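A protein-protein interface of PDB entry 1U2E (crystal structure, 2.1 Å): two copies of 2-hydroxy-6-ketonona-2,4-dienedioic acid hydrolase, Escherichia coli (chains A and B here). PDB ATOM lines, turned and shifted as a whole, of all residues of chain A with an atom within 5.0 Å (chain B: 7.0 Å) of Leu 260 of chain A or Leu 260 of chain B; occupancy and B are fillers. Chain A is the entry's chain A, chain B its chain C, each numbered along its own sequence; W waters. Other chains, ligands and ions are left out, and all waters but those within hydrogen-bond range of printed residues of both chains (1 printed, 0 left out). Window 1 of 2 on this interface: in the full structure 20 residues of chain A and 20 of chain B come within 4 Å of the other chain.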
ATOM      1  N   ILE A 234      34.528  12.217  -4.531  1.00  0.00           N
ATOM      2  CA  ILE A 234      34.897  11.152  -3.611  1.00  0.00           C
ATOM      3  C   ILE A 234      33.742  10.163  -3.544  1.00  0.00           C
ATOM      4  O   ILE A 234      32.586  10.573  -3.406  1.00  0.00           O
ATOM      5  CB  ILE A 234      35.179  11.725  -2.199  1.00  0.00           C
ATOM      6  CG1 ILE A 234      36.167  12.895  -2.314  1.00  0.00           C
ATOM      7  CG2 ILE A 234      35.774  10.640  -1.294  1.00  0.00           C
ATOM      8  CD1 ILE A 234      36.145  13.834  -1.130  1.00  0.00           C
ATOM      9  N   VAL A 235      34.061   8.871  -3.657  1.00  0.00           N
ATOM     10  CA  VAL A 235      33.061   7.810  -3.626  1.00  0.00           C
ATOM     11  C   VAL A 235      33.398   6.817  -2.521  1.00  0.00           C
ATOM     12  O   VAL A 235      34.564   6.479  -2.312  1.00  0.00           O
ATOM     13  CB  VAL A 235      32.993   7.067  -4.986  1.00  0.00           C
ATOM     14  CG1 VAL A 235      31.928   5.982  -4.935  1.00  0.00           C
ATOM     15  CG2 VAL A 235      32.669   8.060  -6.097  1.00  0.00           C
ATOM     16  N   TRP A 236      32.372   6.333  -1.829  1.00  0.00           N
ATOM     17  CA  TRP A 236      32.594   5.419  -0.720  1.00  0.00           C
ATOM     18  C   TRP A 236      31.417   4.502  -0.413  1.00  0.00           C
ATOM     19  O   TRP A 236      30.270   4.781  -0.758  1.00  0.00           O
ATOM     20  CB  TRP A 236      32.912   6.235   0.531  1.00  0.00           C
ATOM     21  CG  TRP A 236      34.060   5.711   1.334  1.00  0.00           C
ATOM     22  CD1 TRP A 236      34.041   4.684   2.240  1.00  0.00           C
ATOM     23  CD2 TRP A 236      35.398   6.222   1.329  1.00  0.00           C
ATOM     24  NE1 TRP A 236      35.290   4.533   2.804  1.00  0.00           N
ATOM     25  CE2 TRP A 236      36.140   5.463   2.262  1.00  0.00           C
ATOM     26  CE3 TRP A 236      36.043   7.255   0.630  1.00  0.00           C
ATOM     27  CZ2 TRP A 236      37.497   5.704   2.515  1.00  0.00           C
ATOM     28  CZ3 TRP A 236      37.397   7.497   0.882  1.00  0.00           C
ATOM     29  CH2 TRP A 236      38.107   6.726   1.817  1.00  0.00           C
ATOM     30  N   GLY A 248      36.351   9.327   4.086  1.00  0.00           N
ATOM     31  CA  GLY A 248      35.762  10.004   2.940  1.00  0.00           C
ATOM     32  C   GLY A 248      35.295  11.392   3.339  1.00  0.00           C
ATOM     33  O   GLY A 248      35.359  12.337   2.543  1.00  0.00           O
ATOM     34  N   LEU A 249      34.816  11.504   4.575  1.00  0.00           N
ATOM     35  CA  LEU A 249      34.358  12.772   5.134  1.00  0.00           C
ATOM     36  C   LEU A 249      35.543  13.731   5.282  1.00  0.00           C
ATOM     37  O   LEU A 249      35.406  14.929   5.049  1.00  0.00           O
ATOM     38  CB  LEU A 249      33.703  12.538   6.499  1.00  0.00           C
ATOM     39  CG  LEU A 249      32.220  12.150   6.584  1.00  0.00           C
ATOM     40  CD1 LEU A 249      31.860  11.226   5.457  1.00  0.00           C
ATOM     41  CD2 LEU A 249      31.933  11.488   7.945  1.00  0.00           C
ATOM     42  N   LEU A 252      36.481  15.097   1.994  1.00  0.00           N
ATOM     43  CA  LEU A 252      35.418  16.047   1.672  1.00  0.00           C
ATOM     44  C   LEU A 252      35.659  17.397   2.352  1.00  0.00           C
ATOM     45  O   LEU A 252      35.636  18.439   1.703  1.00  0.00           O
ATOM     46  CB  LEU A 252      34.070  15.457   2.116  1.00  0.00           C
ATOM     47  CG  LEU A 252      32.693  15.987   1.667  1.00  0.00           C
ATOM     48  CD1 LEU A 252      32.109  16.887   2.718  1.00  0.00           C
ATOM     49  CD2 LEU A 252      32.795  16.682   0.319  1.00  0.00           C
ATOM     50  N   SER A 258      34.952  19.980  -3.493  1.00  0.00           N
ATOM     51  CA  SER A 258      34.744  18.552  -3.700  1.00  0.00           C
ATOM     52  C   SER A 258      33.315  18.087  -3.430  1.00  0.00           C
ATOM     53  O   SER A 258      32.502  18.796  -2.839  1.00  0.00           O
ATOM     54  CB  SER A 258      35.678  17.752  -2.800  1.00  0.00           C
ATOM     55  OG  SER A 258      35.288  17.890  -1.441  1.00  0.00           O
ATOM     56  N   GLU A 259      33.034  16.863  -3.855  1.00  0.00           N
ATOM     57  CA  GLU A 259      31.729  16.261  -3.653  1.00  0.00           C
ATOM     58  C   GLU A 259      31.949  14.838  -3.179  1.00  0.00           C
ATOM     59  O   GLU A 259      32.923  14.201  -3.579  1.00  0.00           O
ATOM     60  CB  GLU A 259      30.937  16.281  -4.962  1.00  0.00           C
ATOM     61  CG  GLU A 259      30.435  17.664  -5.325  1.00  0.00           C
ATOM     62  CD  GLU A 259      29.691  17.700  -6.645  1.00  0.00           C
ATOM     63  OE1 GLU A 259      29.093  16.672  -7.032  1.00  0.00           O
ATOM     64  OE2 GLU A 259      29.689  18.768  -7.288  1.00  0.00           O
ATOM     65  N   LEU A 260      31.058  14.351  -2.318  1.00  0.00           N
ATOM     66  CA  LEU A 260      31.158  12.990  -1.800  1.00  0.00           C
ATOM     67  C   LEU A 260      29.869  12.213  -2.067  1.00  0.00           C
ATOM     68  O   LEU A 260      28.777  12.688  -1.775  1.00  0.00           O
ATOM     69  CB  LEU A 260      31.434  13.014  -0.289  1.00  0.00           C
ATOM     70  CG  LEU A 260      31.342  11.696   0.487  1.00  0.00           C
ATOM     71  CD1 LEU A 260      32.398  10.735  -0.005  1.00  0.00           C
ATOM     72  CD2 LEU A 260      31.542  11.967   1.978  1.00  0.00           C
ATOM     73  N   HIS A 261      29.997  11.013  -2.617  1.00  0.00           N
ATOM     74  CA  HIS A 261      28.824  10.209  -2.879  1.00  0.00           C
ATOM     75  C   HIS A 261      29.026   8.895  -2.133  1.00  0.00           C
ATOM     76  O   HIS A 261      30.002   8.183  -2.364  1.00  0.00           O
ATOM     77  CB  HIS A 261      28.672   9.957  -4.379  1.00  0.00           C
ATOM     78  CG  HIS A 261      27.332   9.408  -4.767  1.00  0.00           C
ATOM     79  ND1 HIS A 261      26.303  10.204  -5.224  1.00  0.00           N
ATOM     80  CD2 HIS A 261      26.846   8.143  -4.747  1.00  0.00           C
ATOM     81  CE1 HIS A 261      25.243   9.454  -5.469  1.00  0.00           C
ATOM     82  NE2 HIS A 261      25.546   8.200  -5.189  1.00  0.00           N
ATOM     83  N   ILE A 262      28.108   8.576  -1.228  1.00  0.00           N
ATOM     84  CA  ILE A 262      28.215   7.344  -0.458  1.00  0.00           C
ATOM     85  C   ILE A 262      27.106   6.359  -0.805  1.00  0.00           C
ATOM     86  O   ILE A 262      25.932   6.728  -0.859  1.00  0.00           O
ATOM     87  CB  ILE A 262      28.118   7.608   1.054  1.00  0.00           C
ATOM     88  CG1 ILE A 262      29.193   8.605   1.494  1.00  0.00           C
ATOM     89  CG2 ILE A 262      28.249   6.291   1.810  1.00  0.00           C
ATOM     90  CD1 ILE A 262      29.027   9.098   2.936  1.00  0.00           C
ATOM     91  N   LEU B 137      15.579  13.207  -0.883  1.00  0.00           N
ATOM     92  CA  LEU B 137      15.605  14.058   0.299  1.00  0.00           C
ATOM     93  C   LEU B 137      16.778  15.029   0.270  1.00  0.00           C
ATOM     94  O   LEU B 137      17.916  14.633   0.007  1.00  0.00           O
ATOM     95  CB  LEU B 137      15.724  13.186   1.561  1.00  0.00           C
ATOM     96  CG  LEU B 137      14.545  12.559   2.317  1.00  0.00           C
ATOM     97  CD1 LEU B 137      13.309  12.429   1.448  1.00  0.00           C
ATOM     98  CD2 LEU B 137      14.997  11.195   2.855  1.00  0.00           C
ATOM     99  N   THR B 232      15.941   5.519  -2.515  1.00  0.00           N
ATOM    100  CA  THR B 232      16.103   6.869  -1.985  1.00  0.00           C
ATOM    101  C   THR B 232      17.451   7.504  -2.301  1.00  0.00           C
ATOM    102  O   THR B 232      18.473   6.821  -2.336  1.00  0.00           O
ATOM    103  CB  THR B 232      15.908   6.829  -0.440  1.00  0.00           C
ATOM    104  OG1 THR B 232      14.616   6.284  -0.147  1.00  0.00           O
ATOM    105  CG2 THR B 232      16.026   8.221   0.178  1.00  0.00           C
ATOM    106  N   LEU B 233      17.431   8.819  -2.523  1.00  0.00           N
ATOM    107  CA  LEU B 233      18.626   9.603  -2.807  1.00  0.00           C
ATOM    108  C   LEU B 233      18.581  10.780  -1.838  1.00  0.00           C
ATOM    109  O   LEU B 233      17.596  11.524  -1.780  1.00  0.00           O
ATOM    110  CB  LEU B 233      18.623  10.113  -4.256  1.00  0.00           C
ATOM    111  CG  LEU B 233      19.885  10.716  -4.904  1.00  0.00           C
ATOM    112  CD1 LEU B 233      19.562  12.100  -5.398  1.00  0.00           C
ATOM    113  CD2 LEU B 233      21.062  10.747  -3.956  1.00  0.00           C
ATOM    114  N   ILE B 234      19.648  10.926  -1.061  1.00  0.00           N
ATOM    115  CA  ILE B 234      19.739  11.991  -0.078  1.00  0.00           C
ATOM    116  C   ILE B 234      20.792  12.984  -0.526  1.00  0.00           C
ATOM    117  O   ILE B 234      21.881  12.590  -0.939  1.00  0.00           O
ATOM    118  CB  ILE B 234      20.126  11.408   1.293  1.00  0.00           C
ATOM    119  CG1 ILE B 234      19.123  10.319   1.674  1.00  0.00           C
ATOM    120  CG2 ILE B 234      20.162  12.516   2.357  1.00  0.00           C
ATOM    121  CD1 ILE B 234      19.694   9.290   2.630  1.00  0.00           C
ATOM    122  N   VAL B 235      20.452  14.270  -0.466  1.00  0.00           N
ATOM    123  CA  VAL B 235      21.375  15.318  -0.865  1.00  0.00           C
ATOM    124  C   VAL B 235      21.564  16.291   0.293  1.00  0.00           C
ATOM    125  O   VAL B 235      20.603  16.670   0.945  1.00  0.00           O
ATOM    126  CB  VAL B 235      20.855  16.073  -2.106  1.00  0.00           C
ATOM    127  CG1 VAL B 235      21.868  17.131  -2.526  1.00  0.00           C
ATOM    128  CG2 VAL B 235      20.601  15.076  -3.255  1.00  0.00           C
ATOM    129  N   TRP B 236      22.806  16.700   0.529  1.00  0.00           N
ATOM    130  CA  TRP B 236      23.120  17.598   1.630  1.00  0.00           C
ATOM    131  C   TRP B 236      24.335  18.466   1.346  1.00  0.00           C
ATOM    132  O   TRP B 236      25.197  18.121   0.526  1.00  0.00           O
ATOM    133  CB  TRP B 236      23.405  16.771   2.890  1.00  0.00           C
ATOM    134  CG  TRP B 236      22.759  17.292   4.140  1.00  0.00           C
ATOM    135  CD1 TRP B 236      23.188  18.322   4.922  1.00  0.00           C
ATOM    136  CD2 TRP B 236      21.549  16.807   4.740  1.00  0.00           C
ATOM    137  NE1 TRP B 236      22.321  18.511   5.979  1.00  0.00           N
ATOM    138  CE2 TRP B 236      21.307  17.593   5.890  1.00  0.00           C
ATOM    139  CE3 TRP B 236      20.649  15.782   4.419  1.00  0.00           C
ATOM    140  CZ2 TRP B 236      20.201  17.387   6.718  1.00  0.00           C
ATOM    141  CZ3 TRP B 236      19.545  15.576   5.248  1.00  0.00           C
ATOM    142  CH2 TRP B 236      19.334  16.376   6.381  1.00  0.00           C
ATOM    143  N   MET B 245      24.715  18.124   8.796  1.00  0.00           N
ATOM    144  CA  MET B 245      24.967  17.106   7.786  1.00  0.00           C
ATOM    145  C   MET B 245      24.853  15.676   8.311  1.00  0.00           C
ATOM    146  O   MET B 245      24.482  14.778   7.561  1.00  0.00           O
ATOM    147  CB  MET B 245      26.362  17.307   7.188  1.00  0.00           C
ATOM    148  CG  MET B 245      26.826  16.164   6.306  1.00  0.00           C
ATOM    149  SD  MET B 245      28.590  16.252   5.995  1.00  0.00           S
ATOM    150  CE  MET B 245      29.229  15.410   7.442  1.00  0.00           C
ATOM    151  N   ALA B 247      22.684  14.506   9.852  1.00  0.00           N
ATOM    152  CA  ALA B 247      21.287  14.098   9.750  1.00  0.00           C
ATOM    153  C   ALA B 247      21.201  13.313   8.440  1.00  0.00           C
ATOM    154  O   ALA B 247      20.460  12.334   8.332  1.00  0.00           O
ATOM    155  CB  ALA B 247      20.366  15.310   9.701  1.00  0.00           C
ATOM    156  N   GLY B 248      21.977  13.749   7.449  1.00  0.00           N
ATOM    157  CA  GLY B 248      22.009  13.060   6.165  1.00  0.00           C
ATOM    158  C   GLY B 248      22.604  11.671   6.361  1.00  0.00           C
ATOM    159  O   GLY B 248      22.167  10.699   5.746  1.00  0.00           O
ATOM    160  N   LEU B 249      23.610  11.581   7.229  1.00  0.00           N
ATOM    161  CA  LEU B 249      24.251  10.302   7.525  1.00  0.00           C
ATOM    162  C   LEU B 249      23.253   9.336   8.179  1.00  0.00           C
ATOM    163  O   LEU B 249      23.280   8.137   7.914  1.00  0.00           O
ATOM    164  CB  LEU B 249      25.448  10.511   8.463  1.00  0.00           C
ATOM    165  CG  LEU B 249      26.863  10.772   7.929  1.00  0.00           C
ATOM    166  CD1 LEU B 249      26.886  10.764   6.419  1.00  0.00           C
ATOM    167  CD2 LEU B 249      27.371  12.089   8.475  1.00  0.00           C
ATOM    168  N   ARG B 250      22.382   9.860   9.039  1.00  0.00           N
ATOM    169  CA  ARG B 250      21.384   9.034   9.718  1.00  0.00           C
ATOM    170  C   ARG B 250      20.402   8.447   8.711  1.00  0.00           C
ATOM    171  O   ARG B 250      20.073   7.263   8.757  1.00  0.00           O
ATOM    172  CB  ARG B 250      20.599   9.861  10.742  1.00  0.00           C
ATOM    173  CG  ARG B 250      21.117   9.777  12.161  1.00  0.00           C
ATOM    174  CD  ARG B 250      19.974   9.481  13.137  1.00  0.00           C
ATOM    175  NE  ARG B 250      18.989  10.561  13.212  1.00  0.00           N
ATOM    176  CZ  ARG B 250      17.778  10.440  13.756  1.00  0.00           C
ATOM    177  NH1 ARG B 250      17.383   9.284  14.278  1.00  0.00           N
ATOM    178  NH2 ARG B 250      16.955  11.481  13.780  1.00  0.00           N
ATOM    179  N   LEU B 251      19.929   9.299   7.810  1.00  0.00           N
ATOM    180  CA  LEU B 251      18.987   8.888   6.788  1.00  0.00           C
ATOM    181  C   LEU B 251      19.623   7.800   5.933  1.00  0.00           C
ATOM    182  O   LEU B 251      18.963   6.829   5.561  1.00  0.00           O
ATOM    183  CB  LEU B 251      18.605  10.097   5.926  1.00  0.00           C
ATOM    184  CG  LEU B 251      17.229  10.772   6.057  1.00  0.00           C
ATOM    185  CD1 LEU B 251      16.490  10.293   7.275  1.00  0.00           C
ATOM    186  CD2 LEU B 251      17.420  12.282   6.087  1.00  0.00           C
ATOM    187  N   LEU B 252      20.909   7.967   5.634  1.00  0.00           N
ATOM    188  CA  LEU B 252      21.653   7.010   4.813  1.00  0.00           C
ATOM    189  C   LEU B 252      21.748   5.649   5.502  1.00  0.00           C
ATOM    190  O   LEU B 252      21.546   4.608   4.875  1.00  0.00           O
ATOM    191  CB  LEU B 252      23.055   7.567   4.526  1.00  0.00           C
ATOM    192  CG  LEU B 252      24.052   6.885   3.579  1.00  0.00           C
ATOM    193  CD1 LEU B 252      24.735   5.764   4.298  1.00  0.00           C
ATOM    194  CD2 LEU B 252      23.353   6.395   2.304  1.00  0.00           C
ATOM    195  N   SER B 258      19.860   3.156  -0.072  1.00  0.00           N
ATOM    196  CA  SER B 258      19.914   4.590  -0.358  1.00  0.00           C
ATOM    197  C   SER B 258      21.327   5.028  -0.710  1.00  0.00           C
ATOM    198  O   SER B 258      22.287   4.274  -0.534  1.00  0.00           O
ATOM    199  CB  SER B 258      19.438   5.413   0.847  1.00  0.00           C
ATOM    200  OG  SER B 258      20.297   5.243   1.966  1.00  0.00           O
ATOM    201  N   GLU B 259      21.437   6.250  -1.222  1.00  0.00           N
ATOM    202  CA  GLU B 259      22.726   6.844  -1.565  1.00  0.00           C
ATOM    203  C   GLU B 259      22.709   8.268  -1.031  1.00  0.00           C
ATOM    204  O   GLU B 259      21.651   8.887  -0.932  1.00  0.00           O
ATOM    205  CB  GLU B 259      22.941   6.850  -3.080  1.00  0.00           C
ATOM    206  CG  GLU B 259      23.345   5.493  -3.646  1.00  0.00           C
ATOM    207  CD  GLU B 259      23.135   5.376  -5.150  1.00  0.00           C
ATOM    208  OE1 GLU B 259      23.400   6.353  -5.887  1.00  0.00           O
ATOM    209  OE2 GLU B 259      22.709   4.292  -5.593  1.00  0.00           O
ATOM    210  N   LEU B 260      23.879   8.780  -0.667  1.00  0.00           N
ATOM    211  CA  LEU B 260      23.979  10.139  -0.148  1.00  0.00           C
ATOM    212  C   LEU B 260      24.988  10.924  -0.981  1.00  0.00           C
ATOM    213  O   LEU B 260      26.086  10.445  -1.247  1.00  0.00           O
ATOM    214  CB  LEU B 260      24.421  10.116   1.325  1.00  0.00           C
ATOM    215  CG  LEU B 260      24.722  11.457   2.019  1.00  0.00           C
ATOM    216  CD1 LEU B 260      23.483  12.309   2.053  1.00  0.00           C
ATOM    217  CD2 LEU B 260      25.213  11.222   3.442  1.00  0.00           C
ATOM    218  N   HIS B 261      24.606  12.115  -1.414  1.00  0.00           N
ATOM    219  CA  HIS B 261      25.517  12.938  -2.186  1.00  0.00           C
ATOM    220  C   HIS B 261      25.697  14.234  -1.405  1.00  0.00           C
ATOM    221  O   HIS B 261      24.725  14.926  -1.116  1.00  0.00           O
ATOM    222  CB  HIS B 261      24.942  13.241  -3.563  1.00  0.00           C
ATOM    223  CG  HIS B 261      25.963  13.747  -4.530  1.00  0.00           C
ATOM    224  ND1 HIS B 261      26.728  12.907  -5.307  1.00  0.00           N
ATOM    225  CD2 HIS B 261      26.406  15.002  -4.782  1.00  0.00           C
ATOM    226  CE1 HIS B 261      27.602  13.621  -5.996  1.00  0.00           C
ATOM    227  NE2 HIS B 261      27.427  14.895  -5.694  1.00  0.00           N
ATOM    228  N   ILE B 262      26.936  14.553  -1.052  1.00  0.00           N
ATOM    229  CA  ILE B 262      27.208  15.759  -0.283  1.00  0.00           C
ATOM    230  C   ILE B 262      28.080  16.749  -1.044  1.00  0.00           C
ATOM    231  O   ILE B 262      29.161  16.398  -1.504  1.00  0.00           O
ATOM    232  CB  ILE B 262      27.949  15.437   1.048  1.00  0.00           C
ATOM    233  CG1 ILE B 262      27.145  14.453   1.903  1.00  0.00           C
ATOM    234  CG2 ILE B 262      28.189  16.726   1.827  1.00  0.00           C
ATOM    235  CD1 ILE B 262      27.926  13.940   3.108  1.00  0.00           C
ATOM    236  N   PHE B 263      27.600  17.985  -1.167  1.00  0.00           N
ATOM    237  CA  PHE B 263      28.360  19.060  -1.808  1.00  0.00           C
ATOM    238  C   PHE B 263      29.081  19.766  -0.662  1.00  0.00           C
ATOM    239  O   PHE B 263      28.430  20.239   0.262  1.00  0.00           O
ATOM    240  CB  PHE B 263      27.421  20.059  -2.488  1.00  0.00           C
ATOM    241  CG  PHE B 263      26.699  19.504  -3.673  1.00  0.00           C
ATOM    242  CD1 PHE B 263      27.352  19.346  -4.891  1.00  0.00           C
ATOM    243  CD2 PHE B 263      25.374  19.098  -3.565  1.00  0.00           C
ATOM    244  CE1 PHE B 263      26.700  18.789  -5.979  1.00  0.00           C
ATOM    245  CE2 PHE B 263      24.712  18.540  -4.652  1.00  0.00           C
ATOM    246  CZ  PHE B 263      25.380  18.385  -5.864  1.00  0.00           C
ATOM    247  N   ARG B 264      30.407  19.828  -0.704  1.00  0.00           N
ATOM    248  CA  ARG B 264      31.161  20.486   0.361  1.00  0.00           C
ATOM    249  C   ARG B 264      30.849  21.981   0.446  1.00  0.00           C
ATOM    250  O   ARG B 264      30.411  22.454   1.488  1.00  0.00           O
ATOM    251  CB  ARG B 264      32.667  20.302   0.157  1.00  0.00           C
ATOM    252  CG  ARG B 264      33.549  21.038   1.182  1.00  0.00           C
ATOM    253  CD  ARG B 264      35.001  21.082   0.698  1.00  0.00           C
ATOM    254  NE  ARG B 264      35.947  21.631   1.670  1.00  0.00           N
ATOM    255  CZ  ARG B 264      36.130  22.928   1.916  1.00  0.00           C
ATOM    256  NH1 ARG B 264      35.426  23.846   1.266  1.00  0.00           N
ATOM    257  NH2 ARG B 264      37.041  23.309   2.804  1.00  0.00           N
HETATM  258  O   HOH W   1      31.681  21.379  -3.405  1.00  0.00           O
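The guanidinium group (NE) of Arg 264 of chain B sits close to the backbone carbonyl oxygen (O) of Leu 252 of chain A. The backbone carbonyl oxygen (O) of Ser 258 of chain A is in hydrogen-bond range of the backbone NH (N) of Arg 264 of chain B (3.2 Å). The side-chain carboxylate (OE1) of Glu 259 of chain A sits at hydrogen-bond distance from a ring nitrogen (NE2) of His 261 of chain B, at 2.8 Å. The backbone NH of Ile 262 of chain B is in hydrogen-bond range of the backbone carbonyl oxygen of Leu 260 of chain A, 2.7 Å away. OE1 of Glu 259 of chain B lies within hydrogen-bond range of NE2 of His 261 of chain A, 2.9 Å away. A ring nitrogen (ND1) of His 261 of chain A lies within hydrogen-bond range of a ring nitrogen (ND1) of His 261 of chain B (2.7 Å). The backbone NH of Ile 262 of chain A is in hydrogen-bond range of the backbone carbonyl oxygen of Leu 260 of chain B, at 2.8 Å.
Glu 259 of chain A touches His 261 of chain B, and with the chains exchanged His 261 of chain A touches Glu 259 of chain B. Glu 259 of chain A touches Ile 262 of chain B, and with the chains exchanged Ile 262 of chain A touches Glu 259 of chain B. Leu 260 of chain A touches its own counterpart, Leu 260 of chain B. Leu 260 of chain A touches His 261 of chain B, and with the chains exchanged His 261 of chain A touches Leu 260 of chain B.
Ile 262 of chain B touches Glu 259 of chain A (O to CA, 3.4 Å). Glu 259 of chain A touches Phe 263 of chain B (CD to CE1, 3.3 Å). Leu 260 of chain A touches Leu 260 of chain B. His 261 of chain B touches Leu 260 of chain A. Leu 260 of chain B touches His 261 of chain A (O to CA, 3.2 Å). O of Ile 262 of chain A touches CA of Glu 259 of chain B, 3.3 Å away.
Water W1 bridges the backbone carbonyl oxygen (O) of Ser 258 of chain A (2.8 Å) and the backbone NH (N) of Arg 264 of chain B (3.4 Å).
Of the 20 printed residues of chain B, 6 touch a printed residue of chain A. Printed residues of chain B that touch a printed residue of chain A: Glu 259, Leu 260, His 261, Ile 262, Phe 263 and Arg 264. Hydrophobic or aromatic side chains of chain B within 4 Å of the printed part of chain A: His 261 and Phe 263. Of the 11 printed residues of chain A, 6 touch a printed residue of chain B. Printed residues of chain A that touch a printed residue of chain B: Leu 252, Ser 258, Glu 259, Leu 260, His 261 and Ile 262. Among the printed residues, 13 pairs touch across the chains.
N of Ile 234 of chain A is in hydrogen-bond range of O of Glu 259 of chain A (2.7 Å). The backbone carbonyl oxygen (O) of Leu 252 of chain A sits at hydrogen-bond distance from the side-chain hydroxyl (OG) of Ser 258 of chain A (3.2 Å). O of Thr 232 of chain B lies within hydrogen-bond range of N of Glu 259 of chain B (3.2 Å). O of Glu 259 of chain B sits at hydrogen-bond distance from N of Ile 234 of chain B (2.9 Å). The backbone NH of His 261 of chain B is in hydrogen-bond range of the backbone carbonyl oxygen of Ile 234 of chain B (2.8 Å). N of Trp 236 of chain B is in hydrogen-bond range of O of His 261 of chain B (3.1 Å).
Leu 260 of chain A touches just these residues of chain B: Leu 260 (3.5 Å), His 261 (3.3 Å) and Ile 262 (2.7 Å). Leu 260 of chain B touches three residues of chain A. Of the printed residues of chain A, Glu 259 of chain B touches His 261 and Ile 262. Printed residues of chain A within 4 Å of Arg 264 of chain B: Leu 252 and Ser 258. Printed residues of chain B within 4 Å of Glu 259 of chain A: His 261, Ile 262 and Phe 263. Of the printed residues of chain B, His 261 of chain A touches Glu 259 (2.9 Å), Leu 260 (3.2 Å) and His 261 (2.7 Å). Of the printed residues of chain B, Ser 258 of chain A touches Arg 264 (3.2 Å). Ile 234 of chain B touches none of the printed residues of chain A. Thr 232 of chain B touches none of the printed residues of chain A. The nearest residue of chain B that does not touch Leu 260 of chain A is Phe 263 of chain B (5.1 Å). The nearest printed residue of chain A that does not touch Leu 260 of chain B is Ile 234 of chain A (6.9 Å).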
